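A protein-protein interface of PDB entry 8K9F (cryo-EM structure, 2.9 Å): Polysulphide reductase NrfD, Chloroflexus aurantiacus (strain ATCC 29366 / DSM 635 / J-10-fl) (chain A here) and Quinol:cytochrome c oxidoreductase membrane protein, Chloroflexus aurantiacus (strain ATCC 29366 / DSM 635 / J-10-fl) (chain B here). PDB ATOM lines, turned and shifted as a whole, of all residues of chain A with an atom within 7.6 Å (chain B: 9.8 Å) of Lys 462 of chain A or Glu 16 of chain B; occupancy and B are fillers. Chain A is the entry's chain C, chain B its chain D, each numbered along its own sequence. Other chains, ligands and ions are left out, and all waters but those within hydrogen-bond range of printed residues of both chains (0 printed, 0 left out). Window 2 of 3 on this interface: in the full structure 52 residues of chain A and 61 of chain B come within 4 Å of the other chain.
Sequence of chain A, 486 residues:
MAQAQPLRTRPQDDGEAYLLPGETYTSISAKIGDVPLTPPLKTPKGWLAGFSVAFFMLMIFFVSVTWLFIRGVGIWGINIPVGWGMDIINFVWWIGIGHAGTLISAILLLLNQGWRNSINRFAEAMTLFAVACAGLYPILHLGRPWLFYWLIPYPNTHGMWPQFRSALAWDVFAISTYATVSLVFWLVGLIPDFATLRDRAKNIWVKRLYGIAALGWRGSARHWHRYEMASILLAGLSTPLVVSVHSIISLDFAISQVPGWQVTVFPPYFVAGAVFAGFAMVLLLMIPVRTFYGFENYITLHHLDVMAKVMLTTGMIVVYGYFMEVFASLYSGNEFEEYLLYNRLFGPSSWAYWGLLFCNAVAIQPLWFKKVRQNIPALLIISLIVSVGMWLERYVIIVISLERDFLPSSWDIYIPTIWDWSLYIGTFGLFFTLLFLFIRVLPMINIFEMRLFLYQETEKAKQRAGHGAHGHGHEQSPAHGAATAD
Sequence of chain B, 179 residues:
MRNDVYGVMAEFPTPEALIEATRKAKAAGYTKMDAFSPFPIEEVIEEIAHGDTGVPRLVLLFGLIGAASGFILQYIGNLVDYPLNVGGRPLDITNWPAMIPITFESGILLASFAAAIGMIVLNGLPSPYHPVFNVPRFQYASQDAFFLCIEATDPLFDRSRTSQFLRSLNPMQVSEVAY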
ATOM      1  N   TYR A  25       1.444  36.657  -6.170  1.00  0.00           N
ATOM      2  CA  TYR A  25       0.155  36.283  -6.761  1.00  0.00           C
ATOM      3  C   TYR A  25      -0.557  37.484  -7.370  1.00  0.00           C
ATOM      4  O   TYR A  25      -1.209  37.361  -8.420  1.00  0.00           O
ATOM      5  CB  TYR A  25      -0.738  35.627  -5.705  1.00  0.00           C
ATOM      6  CG  TYR A  25      -0.018  34.624  -4.837  1.00  0.00           C
ATOM      7  CD1 TYR A  25       0.679  33.566  -5.399  1.00  0.00           C
ATOM      8  CD2 TYR A  25      -0.028  34.744  -3.452  1.00  0.00           C
ATOM      9  CE1 TYR A  25       1.348  32.653  -4.607  1.00  0.00           C
ATOM     10  CE2 TYR A  25       0.633  33.834  -2.654  1.00  0.00           C
ATOM     11  CZ  TYR A  25       1.318  32.792  -3.238  1.00  0.00           C
ATOM     12  OH  TYR A  25       1.979  31.888  -2.444  1.00  0.00           O
ATOM     13  N   TYR A 455       3.572  29.051  -5.610  1.00  0.00           N
ATOM     14  CA  TYR A 455       3.477  28.415  -4.300  1.00  0.00           C
ATOM     15  C   TYR A 455       4.440  27.239  -4.190  1.00  0.00           C
ATOM     16  O   TYR A 455       5.120  27.078  -3.173  1.00  0.00           O
ATOM     17  CB  TYR A 455       2.041  27.941  -4.085  1.00  0.00           C
ATOM     18  CG  TYR A 455       1.730  27.264  -2.763  1.00  0.00           C
ATOM     19  CD1 TYR A 455       2.427  27.567  -1.596  1.00  0.00           C
ATOM     20  CD2 TYR A 455       0.787  26.251  -2.711  1.00  0.00           C
ATOM     21  CE1 TYR A 455       2.149  26.917  -0.418  1.00  0.00           C
ATOM     22  CE2 TYR A 455       0.509  25.599  -1.544  1.00  0.00           C
ATOM     23  CZ  TYR A 455       1.185  25.934  -0.394  1.00  0.00           C
ATOM     24  OH  TYR A 455       0.905  25.276   0.782  1.00  0.00           O
ATOM     25  N   GLN A 456       4.503  26.404  -5.226  1.00  0.00           N
ATOM     26  CA  GLN A 456       5.374  25.235  -5.192  1.00  0.00           C
ATOM     27  C   GLN A 456       6.838  25.642  -5.231  1.00  0.00           C
ATOM     28  O   GLN A 456       7.679  25.015  -4.577  1.00  0.00           O
ATOM     29  CB  GLN A 456       5.033  24.304  -6.354  1.00  0.00           C
ATOM     30  CG  GLN A 456       3.736  23.536  -6.150  1.00  0.00           C
ATOM     31  CD  GLN A 456       3.280  22.817  -7.397  1.00  0.00           C
ATOM     32  OE1 GLN A 456       3.688  23.156  -8.507  1.00  0.00           O
ATOM     33  NE2 GLN A 456       2.426  21.818  -7.224  1.00  0.00           N
ATOM     34  N   GLU A 457       7.152  26.715  -5.956  1.00  0.00           N
ATOM     35  CA  GLU A 457       8.520  27.213  -6.001  1.00  0.00           C
ATOM     36  C   GLU A 457       8.945  27.807  -4.665  1.00  0.00           C
ATOM     37  O   GLU A 457      10.055  27.537  -4.193  1.00  0.00           O
ATOM     38  CB  GLU A 457       8.665  28.239  -7.122  1.00  0.00           C
ATOM     39  CG  GLU A 457       8.887  27.621  -8.483  1.00  0.00           C
ATOM     40  CD  GLU A 457      10.330  27.712  -8.929  1.00  0.00           C
ATOM     41  OE1 GLU A 457      10.697  27.027  -9.905  1.00  0.00           O
ATOM     42  OE2 GLU A 457      11.100  28.470  -8.302  1.00  0.00           O
ATOM     43  N   THR A 458       8.077  28.590  -4.017  1.00  0.00           N
ATOM     44  CA  THR A 458       8.471  29.134  -2.721  1.00  0.00           C
ATOM     45  C   THR A 458       8.419  28.071  -1.629  1.00  0.00           C
ATOM     46  O   THR A 458       9.084  28.214  -0.600  1.00  0.00           O
ATOM     47  CB  THR A 458       7.617  30.345  -2.330  1.00  0.00           C
ATOM     48  OG1 THR A 458       8.099  30.877  -1.091  1.00  0.00           O
ATOM     49  CG2 THR A 458       6.173  29.971  -2.132  1.00  0.00           C
ATOM     50  N   GLU A 459       7.664  26.990  -1.841  1.00  0.00           N
ATOM     51  CA  GLU A 459       7.658  25.901  -0.872  1.00  0.00           C
ATOM     52  C   GLU A 459       8.915  25.050  -1.002  1.00  0.00           C
ATOM     53  O   GLU A 459       9.460  24.586   0.004  1.00  0.00           O
ATOM     54  CB  GLU A 459       6.397  25.059  -1.054  1.00  0.00           C
ATOM     55  CG  GLU A 459       6.017  24.215   0.150  1.00  0.00           C
ATOM     56  CD  GLU A 459       5.365  25.018   1.268  1.00  0.00           C
ATOM     57  OE1 GLU A 459       4.983  26.187   1.037  1.00  0.00           O
ATOM     58  OE2 GLU A 459       5.235  24.474   2.385  1.00  0.00           O
ATOM     59  N   LYS A 460       9.393  24.843  -2.234  1.00  0.00           N
ATOM     60  CA  LYS A 460      10.704  24.240  -2.444  1.00  0.00           C
ATOM     61  C   LYS A 460      11.792  25.138  -1.857  1.00  0.00           C
ATOM     62  O   LYS A 460      12.733  24.651  -1.223  1.00  0.00           O
ATOM     63  CB  LYS A 460      10.899  23.989  -3.950  1.00  0.00           C
ATOM     64  CG  LYS A 460      12.308  23.725  -4.585  1.00  0.00           C
ATOM     65  CD  LYS A 460      13.322  22.854  -3.820  1.00  0.00           C
ATOM     66  CE  LYS A 460      14.740  23.096  -4.338  1.00  0.00           C
ATOM     67  NZ  LYS A 460      15.778  23.071  -3.267  1.00  0.00           N
ATOM     68  N   ALA A 461      11.656  26.456  -2.020  1.00  0.00           N
ATOM     69  CA  ALA A 461      12.579  27.385  -1.378  1.00  0.00           C
ATOM     70  C   ALA A 461      12.447  27.392   0.144  1.00  0.00           C
ATOM     71  O   ALA A 461      13.369  27.849   0.826  1.00  0.00           O
ATOM     72  CB  ALA A 461      12.365  28.793  -1.926  1.00  0.00           C
ATOM     73  N   LYS A 462      11.328  26.908   0.691  1.00  0.00           N
ATOM     74  CA  LYS A 462      11.207  26.784   2.139  1.00  0.00           C
ATOM     75  C   LYS A 462      11.848  25.495   2.649  1.00  0.00           C
ATOM     76  O   LYS A 462      12.756  25.540   3.487  1.00  0.00           O
ATOM     77  CB  LYS A 462       9.737  26.859   2.562  1.00  0.00           C
ATOM     78  CG  LYS A 462       9.356  28.177   3.224  1.00  0.00           C
ATOM     79  CD  LYS A 462       7.853  28.354   3.321  1.00  0.00           C
ATOM     80  CE  LYS A 462       7.490  29.443   4.324  1.00  0.00           C
ATOM     81  NZ  LYS A 462       6.342  29.065   5.201  1.00  0.00           N
ATOM     82  N   GLN A 463      11.402  24.335   2.152  1.00  0.00           N
ATOM     83  CA  GLN A 463      11.931  23.065   2.642  1.00  0.00           C
ATOM     84  C   GLN A 463      13.333  22.747   2.135  1.00  0.00           C
ATOM     85  O   GLN A 463      13.949  21.811   2.662  1.00  0.00           O
ATOM     86  CB  GLN A 463      11.006  21.894   2.286  1.00  0.00           C
ATOM     87  CG  GLN A 463       9.860  21.672   3.266  1.00  0.00           C
ATOM     88  CD  GLN A 463       8.500  21.993   2.690  1.00  0.00           C
ATOM     89  OE1 GLN A 463       8.393  22.493   1.583  1.00  0.00           O
ATOM     90  NE2 GLN A 463       7.453  21.710   3.451  1.00  0.00           N
ATOM     91  N   ARG A 464      13.835  23.496   1.150  1.00  0.00           N
ATOM     92  CA  ARG A 464      15.153  23.309   0.522  1.00  0.00           C
ATOM     93  C   ARG A 464      15.347  21.896  -0.027  1.00  0.00           C
ATOM     94  O   ARG A 464      14.639  21.472  -0.941  1.00  0.00           O
ATOM     95  CB  ARG A 464      16.284  23.659   1.498  1.00  0.00           C
ATOM     96  CG  ARG A 464      16.388  25.137   1.833  1.00  0.00           C
ATOM     97  CD  ARG A 464      17.703  25.446   2.537  1.00  0.00           C
ATOM     98  NE  ARG A 464      17.816  24.763   3.819  1.00  0.00           N
ATOM     99  CZ  ARG A 464      17.339  25.234   4.962  1.00  0.00           C
ATOM    100  NH1 ARG A 464      16.716  26.400   5.024  1.00  0.00           N
ATOM    101  NH2 ARG A 464      17.494  24.518   6.073  1.00  0.00           N
ATOM    102  N   PHE B  12      -7.654  35.586   5.234  1.00  0.00           N
ATOM    103  CA  PHE B  12      -6.261  35.473   5.658  1.00  0.00           C
ATOM    104  C   PHE B  12      -5.297  35.912   4.552  1.00  0.00           C
ATOM    105  O   PHE B  12      -5.561  35.691   3.367  1.00  0.00           O
ATOM    106  CB  PHE B  12      -5.954  34.040   6.065  1.00  0.00           C
ATOM    107  CG  PHE B  12      -6.778  33.560   7.212  1.00  0.00           C
ATOM    108  CD1 PHE B  12      -6.597  34.085   8.477  1.00  0.00           C
ATOM    109  CD2 PHE B  12      -7.744  32.597   7.021  1.00  0.00           C
ATOM    110  CE1 PHE B  12      -7.362  33.648   9.535  1.00  0.00           C
ATOM    111  CE2 PHE B  12      -8.501  32.154   8.070  1.00  0.00           C
ATOM    112  CZ  PHE B  12      -8.321  32.688   9.328  1.00  0.00           C
ATOM    113  N   PRO B  13      -4.162  36.549   4.917  1.00  0.00           N
ATOM    114  CA  PRO B  13      -3.248  37.102   3.898  1.00  0.00           C
ATOM    115  C   PRO B  13      -2.501  36.108   3.020  1.00  0.00           C
ATOM    116  O   PRO B  13      -2.573  36.188   1.790  1.00  0.00           O
ATOM    117  CB  PRO B  13      -2.250  37.914   4.737  1.00  0.00           C
ATOM    118  CG  PRO B  13      -2.353  37.366   6.112  1.00  0.00           C
ATOM    119  CD  PRO B  13      -3.777  36.963   6.278  1.00  0.00           C
ATOM    120  N   THR B  14      -1.767  35.185   3.630  1.00  0.00           N
ATOM    121  CA  THR B  14      -0.849  34.300   2.935  1.00  0.00           C
ATOM    122  C   THR B  14      -1.425  32.888   2.891  1.00  0.00           C
ATOM    123  O   THR B  14      -2.281  32.555   3.717  1.00  0.00           O
ATOM    124  CB  THR B  14       0.520  34.286   3.634  1.00  0.00           C
ATOM    125  OG1 THR B  14       0.542  33.267   4.640  1.00  0.00           O
ATOM    126  CG2 THR B  14       0.809  35.633   4.270  1.00  0.00           C
ATOM    127  N   PRO B  15      -1.035  32.054   1.916  1.00  0.00           N
ATOM    128  CA  PRO B  15      -1.509  30.659   1.933  1.00  0.00           C
ATOM    129  C   PRO B  15      -1.040  29.871   3.143  1.00  0.00           C
ATOM    130  O   PRO B  15      -1.790  29.020   3.628  1.00  0.00           O
ATOM    131  CB  PRO B  15      -0.959  30.069   0.626  1.00  0.00           C
ATOM    132  CG  PRO B  15       0.054  31.013   0.143  1.00  0.00           C
ATOM    133  CD  PRO B  15      -0.249  32.354   0.705  1.00  0.00           C
ATOM    134  N   GLU B  16       0.159  30.153   3.661  1.00  0.00           N
ATOM    135  CA  GLU B  16       0.633  29.481   4.869  1.00  0.00           C
ATOM    136  C   GLU B  16      -0.155  29.921   6.093  1.00  0.00           C
ATOM    137  O   GLU B  16      -0.384  29.120   7.010  1.00  0.00           O
ATOM    138  CB  GLU B  16       2.121  29.752   5.087  1.00  0.00           C
ATOM    139  CG  GLU B  16       3.045  29.011   4.140  1.00  0.00           C
ATOM    140  CD  GLU B  16       3.175  29.715   2.812  1.00  0.00           C
ATOM    141  OE1 GLU B  16       3.376  30.948   2.814  1.00  0.00           O
ATOM    142  OE2 GLU B  16       3.064  29.039   1.769  1.00  0.00           O
ATOM    143  N   ALA B  17      -0.561  31.195   6.135  1.00  0.00           N
ATOM    144  CA  ALA B  17      -1.435  31.659   7.207  1.00  0.00           C
ATOM    145  C   ALA B  17      -2.794  30.984   7.134  1.00  0.00           C
ATOM    146  O   ALA B  17      -3.358  30.614   8.166  1.00  0.00           O
ATOM    147  CB  ALA B  17      -1.592  33.178   7.152  1.00  0.00           C
ATOM    148  N   LEU B  18      -3.316  30.792   5.917  1.00  0.00           N
ATOM    149  CA  LEU B  18      -4.568  30.062   5.738  1.00  0.00           C
ATOM    150  C   LEU B  18      -4.420  28.606   6.155  1.00  0.00           C
ATOM    151  O   LEU B  18      -5.351  28.019   6.713  1.00  0.00           O
ATOM    152  CB  LEU B  18      -5.030  30.157   4.282  1.00  0.00           C
ATOM    153  CG  LEU B  18      -6.288  29.383   3.871  1.00  0.00           C
ATOM    154  CD1 LEU B  18      -7.550  30.056   4.377  1.00  0.00           C
ATOM    155  CD2 LEU B  18      -6.344  29.198   2.367  1.00  0.00           C
ATOM    156  N   ILE B  19      -3.243  28.018   5.928  1.00  0.00           N
ATOM    157  CA  ILE B  19      -3.033  26.614   6.281  1.00  0.00           C
ATOM    158  C   ILE B  19      -2.945  26.436   7.788  1.00  0.00           C
ATOM    159  O   ILE B  19      -3.601  25.553   8.359  1.00  0.00           O
ATOM    160  CB  ILE B  19      -1.791  26.062   5.558  1.00  0.00           C
ATOM    161  CG1 ILE B  19      -2.095  25.835   4.074  1.00  0.00           C
ATOM    162  CG2 ILE B  19      -1.306  24.765   6.193  1.00  0.00           C
ATOM    163  CD1 ILE B  19      -3.525  25.430   3.774  1.00  0.00           C
ATOM    164  N   GLU B  20      -2.149  27.276   8.460  1.00  0.00           N
ATOM    165  CA  GLU B  20      -2.074  27.222   9.916  1.00  0.00           C
ATOM    166  C   GLU B  20      -3.401  27.609  10.551  1.00  0.00           C
ATOM    167  O   GLU B  20      -3.751  27.104  11.624  1.00  0.00           O
ATOM    168  CB  GLU B  20      -0.957  28.134  10.419  1.00  0.00           C
ATOM    169  CG  GLU B  20       0.440  27.675  10.034  1.00  0.00           C
ATOM    170  CD  GLU B  20       1.525  28.639  10.486  1.00  0.00           C
ATOM    171  OE1 GLU B  20       1.180  29.757  10.932  1.00  0.00           O
ATOM    172  OE2 GLU B  20       2.721  28.292  10.367  1.00  0.00           O
ATOM    173  N   ALA B  21      -4.175  28.453   9.871  1.00  0.00           N
ATOM    174  CA  ALA B  21      -5.493  28.824  10.352  1.00  0.00           C
ATOM    175  C   ALA B  21      -6.479  27.672  10.253  1.00  0.00           C
ATOM    176  O   ALA B  21      -7.230  27.405  11.197  1.00  0.00           O
ATOM    177  CB  ALA B  21      -5.994  30.022   9.558  1.00  0.00           C
ATOM    178  N   THR B  22      -6.499  26.987   9.111  1.00  0.00           N
ATOM    179  CA  THR B  22      -7.418  25.878   8.905  1.00  0.00           C
ATOM    180  C   THR B  22      -7.001  24.661   9.719  1.00  0.00           C
ATOM    181  O   THR B  22      -7.829  23.796  10.017  1.00  0.00           O
ATOM    182  CB  THR B  22      -7.486  25.569   7.411  1.00  0.00           C
ATOM    183  OG1 THR B  22      -7.550  26.805   6.690  1.00  0.00           O
ATOM    184  CG2 THR B  22      -8.711  24.754   7.066  1.00  0.00           C
ATOM    185  N   ARG B  23      -5.726  24.580  10.096  1.00  0.00           N
ATOM    186  CA  ARG B  23      -5.320  23.587  11.080  1.00  0.00           C
ATOM    187  C   ARG B  23      -5.781  23.989  12.477  1.00  0.00           C
ATOM    188  O   ARG B  23      -6.170  23.132  13.277  1.00  0.00           O
ATOM    189  CB  ARG B  23      -3.802  23.398  11.059  1.00  0.00           C
ATOM    190  CG  ARG B  23      -3.296  22.340  12.026  1.00  0.00           C
ATOM    191  CD  ARG B  23      -1.784  22.185  12.039  1.00  0.00           C
ATOM    192  NE  ARG B  23      -1.113  23.384  12.532  1.00  0.00           N
ATOM    193  CZ  ARG B  23       0.168  23.656  12.336  1.00  0.00           C
ATOM    194  NH1 ARG B  23       0.930  22.813  11.649  1.00  0.00           N
ATOM    195  NH2 ARG B  23       0.694  24.772  12.822  1.00  0.00           N
ATOM    196  N   LYS B  24      -5.748  25.289  12.786  1.00  0.00           N
ATOM    197  CA  LYS B  24      -6.314  25.754  14.049  1.00  0.00           C
ATOM    198  C   LYS B  24      -7.832  25.643  14.050  1.00  0.00           C
ATOM    199  O   LYS B  24      -8.432  25.298  15.074  1.00  0.00           O
ATOM    200  CB  LYS B  24      -5.879  27.192  14.331  1.00  0.00           C
ATOM    201  CG  LYS B  24      -4.456  27.310  14.832  1.00  0.00           C
ATOM    202  CD  LYS B  24      -4.087  28.744  15.159  1.00  0.00           C
ATOM    203  CE  LYS B  24      -2.608  28.856  15.471  1.00  0.00           C
ATOM    204  NZ  LYS B  24      -2.147  27.746  16.352  1.00  0.00           N
ATOM    205  N   SER B  37      -9.597  30.146  -2.155  1.00  0.00           N
ATOM    206  CA  SER B  37      -8.208  30.297  -2.567  1.00  0.00           C
ATOM    207  C   SER B  37      -8.163  30.586  -4.059  1.00  0.00           C
ATOM    208  O   SER B  37      -9.046  30.138  -4.796  1.00  0.00           O
ATOM    209  CB  SER B  37      -7.408  29.028  -2.249  1.00  0.00           C
ATOM    210  OG  SER B  37      -7.200  28.872  -0.859  1.00  0.00           O
ATOM    211  N   PHE B  39      -5.776  29.367  -5.950  1.00  0.00           N
ATOM    212  CA  PHE B  39      -5.114  28.191  -6.488  1.00  0.00           C
ATOM    213  C   PHE B  39      -5.272  27.075  -5.468  1.00  0.00           C
ATOM    214  O   PHE B  39      -5.486  27.347  -4.283  1.00  0.00           O
ATOM    215  CB  PHE B  39      -3.630  28.473  -6.782  1.00  0.00           C
ATOM    216  CG  PHE B  39      -2.864  29.044  -5.622  1.00  0.00           C
ATOM    217  CD1 PHE B  39      -2.797  30.413  -5.422  1.00  0.00           C
ATOM    218  CD2 PHE B  39      -2.175  28.216  -4.756  1.00  0.00           C
ATOM    219  CE1 PHE B  39      -2.086  30.936  -4.376  1.00  0.00           C
ATOM    220  CE2 PHE B  39      -1.462  28.737  -3.705  1.00  0.00           C
ATOM    221  CZ  PHE B  39      -1.419  30.099  -3.514  1.00  0.00           C
ATOM    222  N   ILE B  41      -4.338  24.895  -2.714  1.00  0.00           N
ATOM    223  CA  ILE B  41      -3.237  24.888  -1.760  1.00  0.00           C
ATOM    224  C   ILE B  41      -2.735  23.468  -1.518  1.00  0.00           C
ATOM    225  O   ILE B  41      -1.562  23.265  -1.176  1.00  0.00           O
ATOM    226  CB  ILE B  41      -3.683  25.560  -0.452  1.00  0.00           C
ATOM    227  CG1 ILE B  41      -4.601  26.751  -0.753  1.00  0.00           C
ATOM    228  CG2 ILE B  41      -2.477  26.013   0.342  1.00  0.00           C
ATOM    229  CD1 ILE B  41      -3.890  28.017  -1.156  1.00  0.00           C
ATOM    230  N   GLU B  43      -3.442  21.705   0.949  1.00  0.00           N
ATOM    231  CA  GLU B  43      -3.303  21.461   2.376  1.00  0.00           C
ATOM    232  C   GLU B  43      -4.596  21.805   3.113  1.00  0.00           C
ATOM    233  O   GLU B  43      -4.890  21.200   4.145  1.00  0.00           O
ATOM    234  CB  GLU B  43      -2.110  22.231   2.928  1.00  0.00           C
ATOM    235  CG  GLU B  43      -0.775  21.779   2.380  1.00  0.00           C
ATOM    236  CD  GLU B  43      -0.523  20.314   2.645  1.00  0.00           C
ATOM    237  OE1 GLU B  43      -0.858  19.842   3.749  1.00  0.00           O
ATOM    238  OE2 GLU B  43       0.004  19.635   1.739  1.00  0.00           O
ATOM    239  N   VAL B  44      -5.369  22.780   2.619  1.00  0.00           N
ATOM    240  CA  VAL B  44      -6.788  22.817   2.973  1.00  0.00           C
ATOM    241  C   VAL B  44      -7.521  21.667   2.301  1.00  0.00           C
ATOM    242  O   VAL B  44      -8.374  21.012   2.910  1.00  0.00           O
ATOM    243  CB  VAL B  44      -7.434  24.175   2.623  1.00  0.00           C
ATOM    244  CG1 VAL B  44      -7.154  25.201   3.686  1.00  0.00           C
ATOM    245  CG2 VAL B  44      -6.924  24.692   1.293  1.00  0.00           C
ATOM    246  N   ALA B 145      -6.333  36.305  -2.673  1.00  0.00           N
ATOM    247  CA  ALA B 145      -6.775  36.256  -1.280  1.00  0.00           C
ATOM    248  C   ALA B 145      -7.102  34.889  -0.824  1.00  0.00           C
ATOM    249  O   ALA B 145      -7.399  34.016  -1.620  1.00  0.00           O
ATOM    250  CB  ALA B 145      -7.916  37.194  -0.970  1.00  0.00           C
ATOM    251  N   PHE B 146      -7.037  34.689   0.475  1.00  0.00           N
ATOM    252  CA  PHE B 146      -7.246  33.378   0.986  1.00  0.00           C
ATOM    253  C   PHE B 146      -8.301  33.472   2.038  1.00  0.00           C
ATOM    254  O   PHE B 146      -8.087  34.036   3.092  1.00  0.00           O
ATOM    255  CB  PHE B 146      -5.940  32.783   1.458  1.00  0.00           C
ATOM    256  CG  PHE B 146      -4.895  32.747   0.398  1.00  0.00           C
ATOM    257  CD1 PHE B 146      -4.077  33.840   0.176  1.00  0.00           C
ATOM    258  CD2 PHE B 146      -4.757  31.639  -0.407  1.00  0.00           C
ATOM    259  CE1 PHE B 146      -3.136  33.829  -0.824  1.00  0.00           C
ATOM    260  CE2 PHE B 146      -3.810  31.613  -1.399  1.00  0.00           C
ATOM    261  CZ  PHE B 146      -3.001  32.711  -1.611  1.00  0.00           C
ATOM    262  N   LEU B 169      -7.836  33.702  16.064  1.00  0.00           N
ATOM    263  CA  LEU B 169      -6.690  33.603  15.179  1.00  0.00           C
ATOM    264  C   LEU B 169      -6.696  34.799  14.229  1.00  0.00           C
ATOM    265  O   LEU B 169      -7.734  35.135  13.653  1.00  0.00           O
ATOM    266  CB  LEU B 169      -6.709  32.288  14.395  1.00  0.00           C
ATOM    267  CG  LEU B 169      -7.901  32.075  13.460  1.00  0.00           C
ATOM    268  CD1 LEU B 169      -7.702  32.831  12.156  1.00  0.00           C
ATOM    269  CD2 LEU B 169      -8.120  30.593  13.198  1.00  0.00           C
ATOM    270  N   ASN B 170      -5.540  35.450  14.089  1.00  0.00           N
ATOM    271  CA  ASN B 170      -5.489  36.848  13.653  1.00  0.00           C
ATOM    272  C   ASN B 170      -5.815  37.002  12.171  1.00  0.00           C
ATOM    273  O   ASN B 170      -5.068  36.500  11.323  1.00  0.00           O
ATOM    274  CB  ASN B 170      -4.116  37.435  13.948  1.00  0.00           C
ATOM    275  CG  ASN B 170      -2.993  36.455  13.673  1.00  0.00           C
ATOM    276  OD1 ASN B 170      -2.939  35.377  14.262  1.00  0.00           O
ATOM    277  ND2 ASN B 170      -2.094  36.821  12.766  1.00  0.00           N
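Pro 15 of chain B touches Tyr 25 of chain A (CG to OH, 3.3 Å).
Phe 39 of chain B touches Tyr 25 of chain A.
Tyr 25 of chain A touches Phe 146 of chain B (CE2 to CZ, 3.9 Å).
Tyr 455 of chain A touches Glu 16 of chain B (CE1 to OE2, 3.2 Å).
Tyr 455 of chain A touches Phe 39 of chain B (CD2 to CE2, 3.5 Å).
Ile 41 of chain B touches Tyr 455 of chain A.
Glu 16 of chain B touches Glu 459 of chain A (OE2 to OE1, 3.5 Å).
NZ of Lys 462 of chain A touches CG of Glu 16 of chain B (3.5 Å).
Lys 462 of chain A touches just one residue of chain B: Glu 16.
Glu 16 of chain B touches three residues of chain A.
Of the printed residues of chain A, Pro 15 of chain B touches Tyr 25.
Of the printed residues of chain A, Phe 39 of chain B touches Tyr 25 (3.8 Å) and Tyr 455 (3.5 Å).
Of the printed residues of chain B, Tyr 455 of chain A touches Glu 16, Phe 39 and Ile 41.
Thr 22 of chain B touches none of the printed residues of chain A.
Ala 17 of chain B touches none of the printed residues of chain A.
The nearest residue of chain A that does not touch Glu 16 of chain B is Thr 458 of chain A (5.1 Å).
Hydrophobic or aromatic side chains of chain A that line the printed part of chain B: Tyr 25 and Tyr 455.
Of the 22 printed residues of chain B, 5 touch a printed residue of chain A.
Among the printed residues, 8 pairs touch across the chains.
The backbone NH of Phe 12 of chain B sits at hydrogen-bond distance from the backbone carbonyl oxygen of Phe 146 of chain B (2.7 Å).
The side-chain hydroxyl of Thr 14 of chain B sits close to the backbone NH of Glu 16 of chain B (3.3 Å).
The backbone carbonyl oxygen (O) of Glu 459 of chain A sits close to the side-chain amide oxygen (OE1) of Gln 463 of chain A (2.8 Å).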
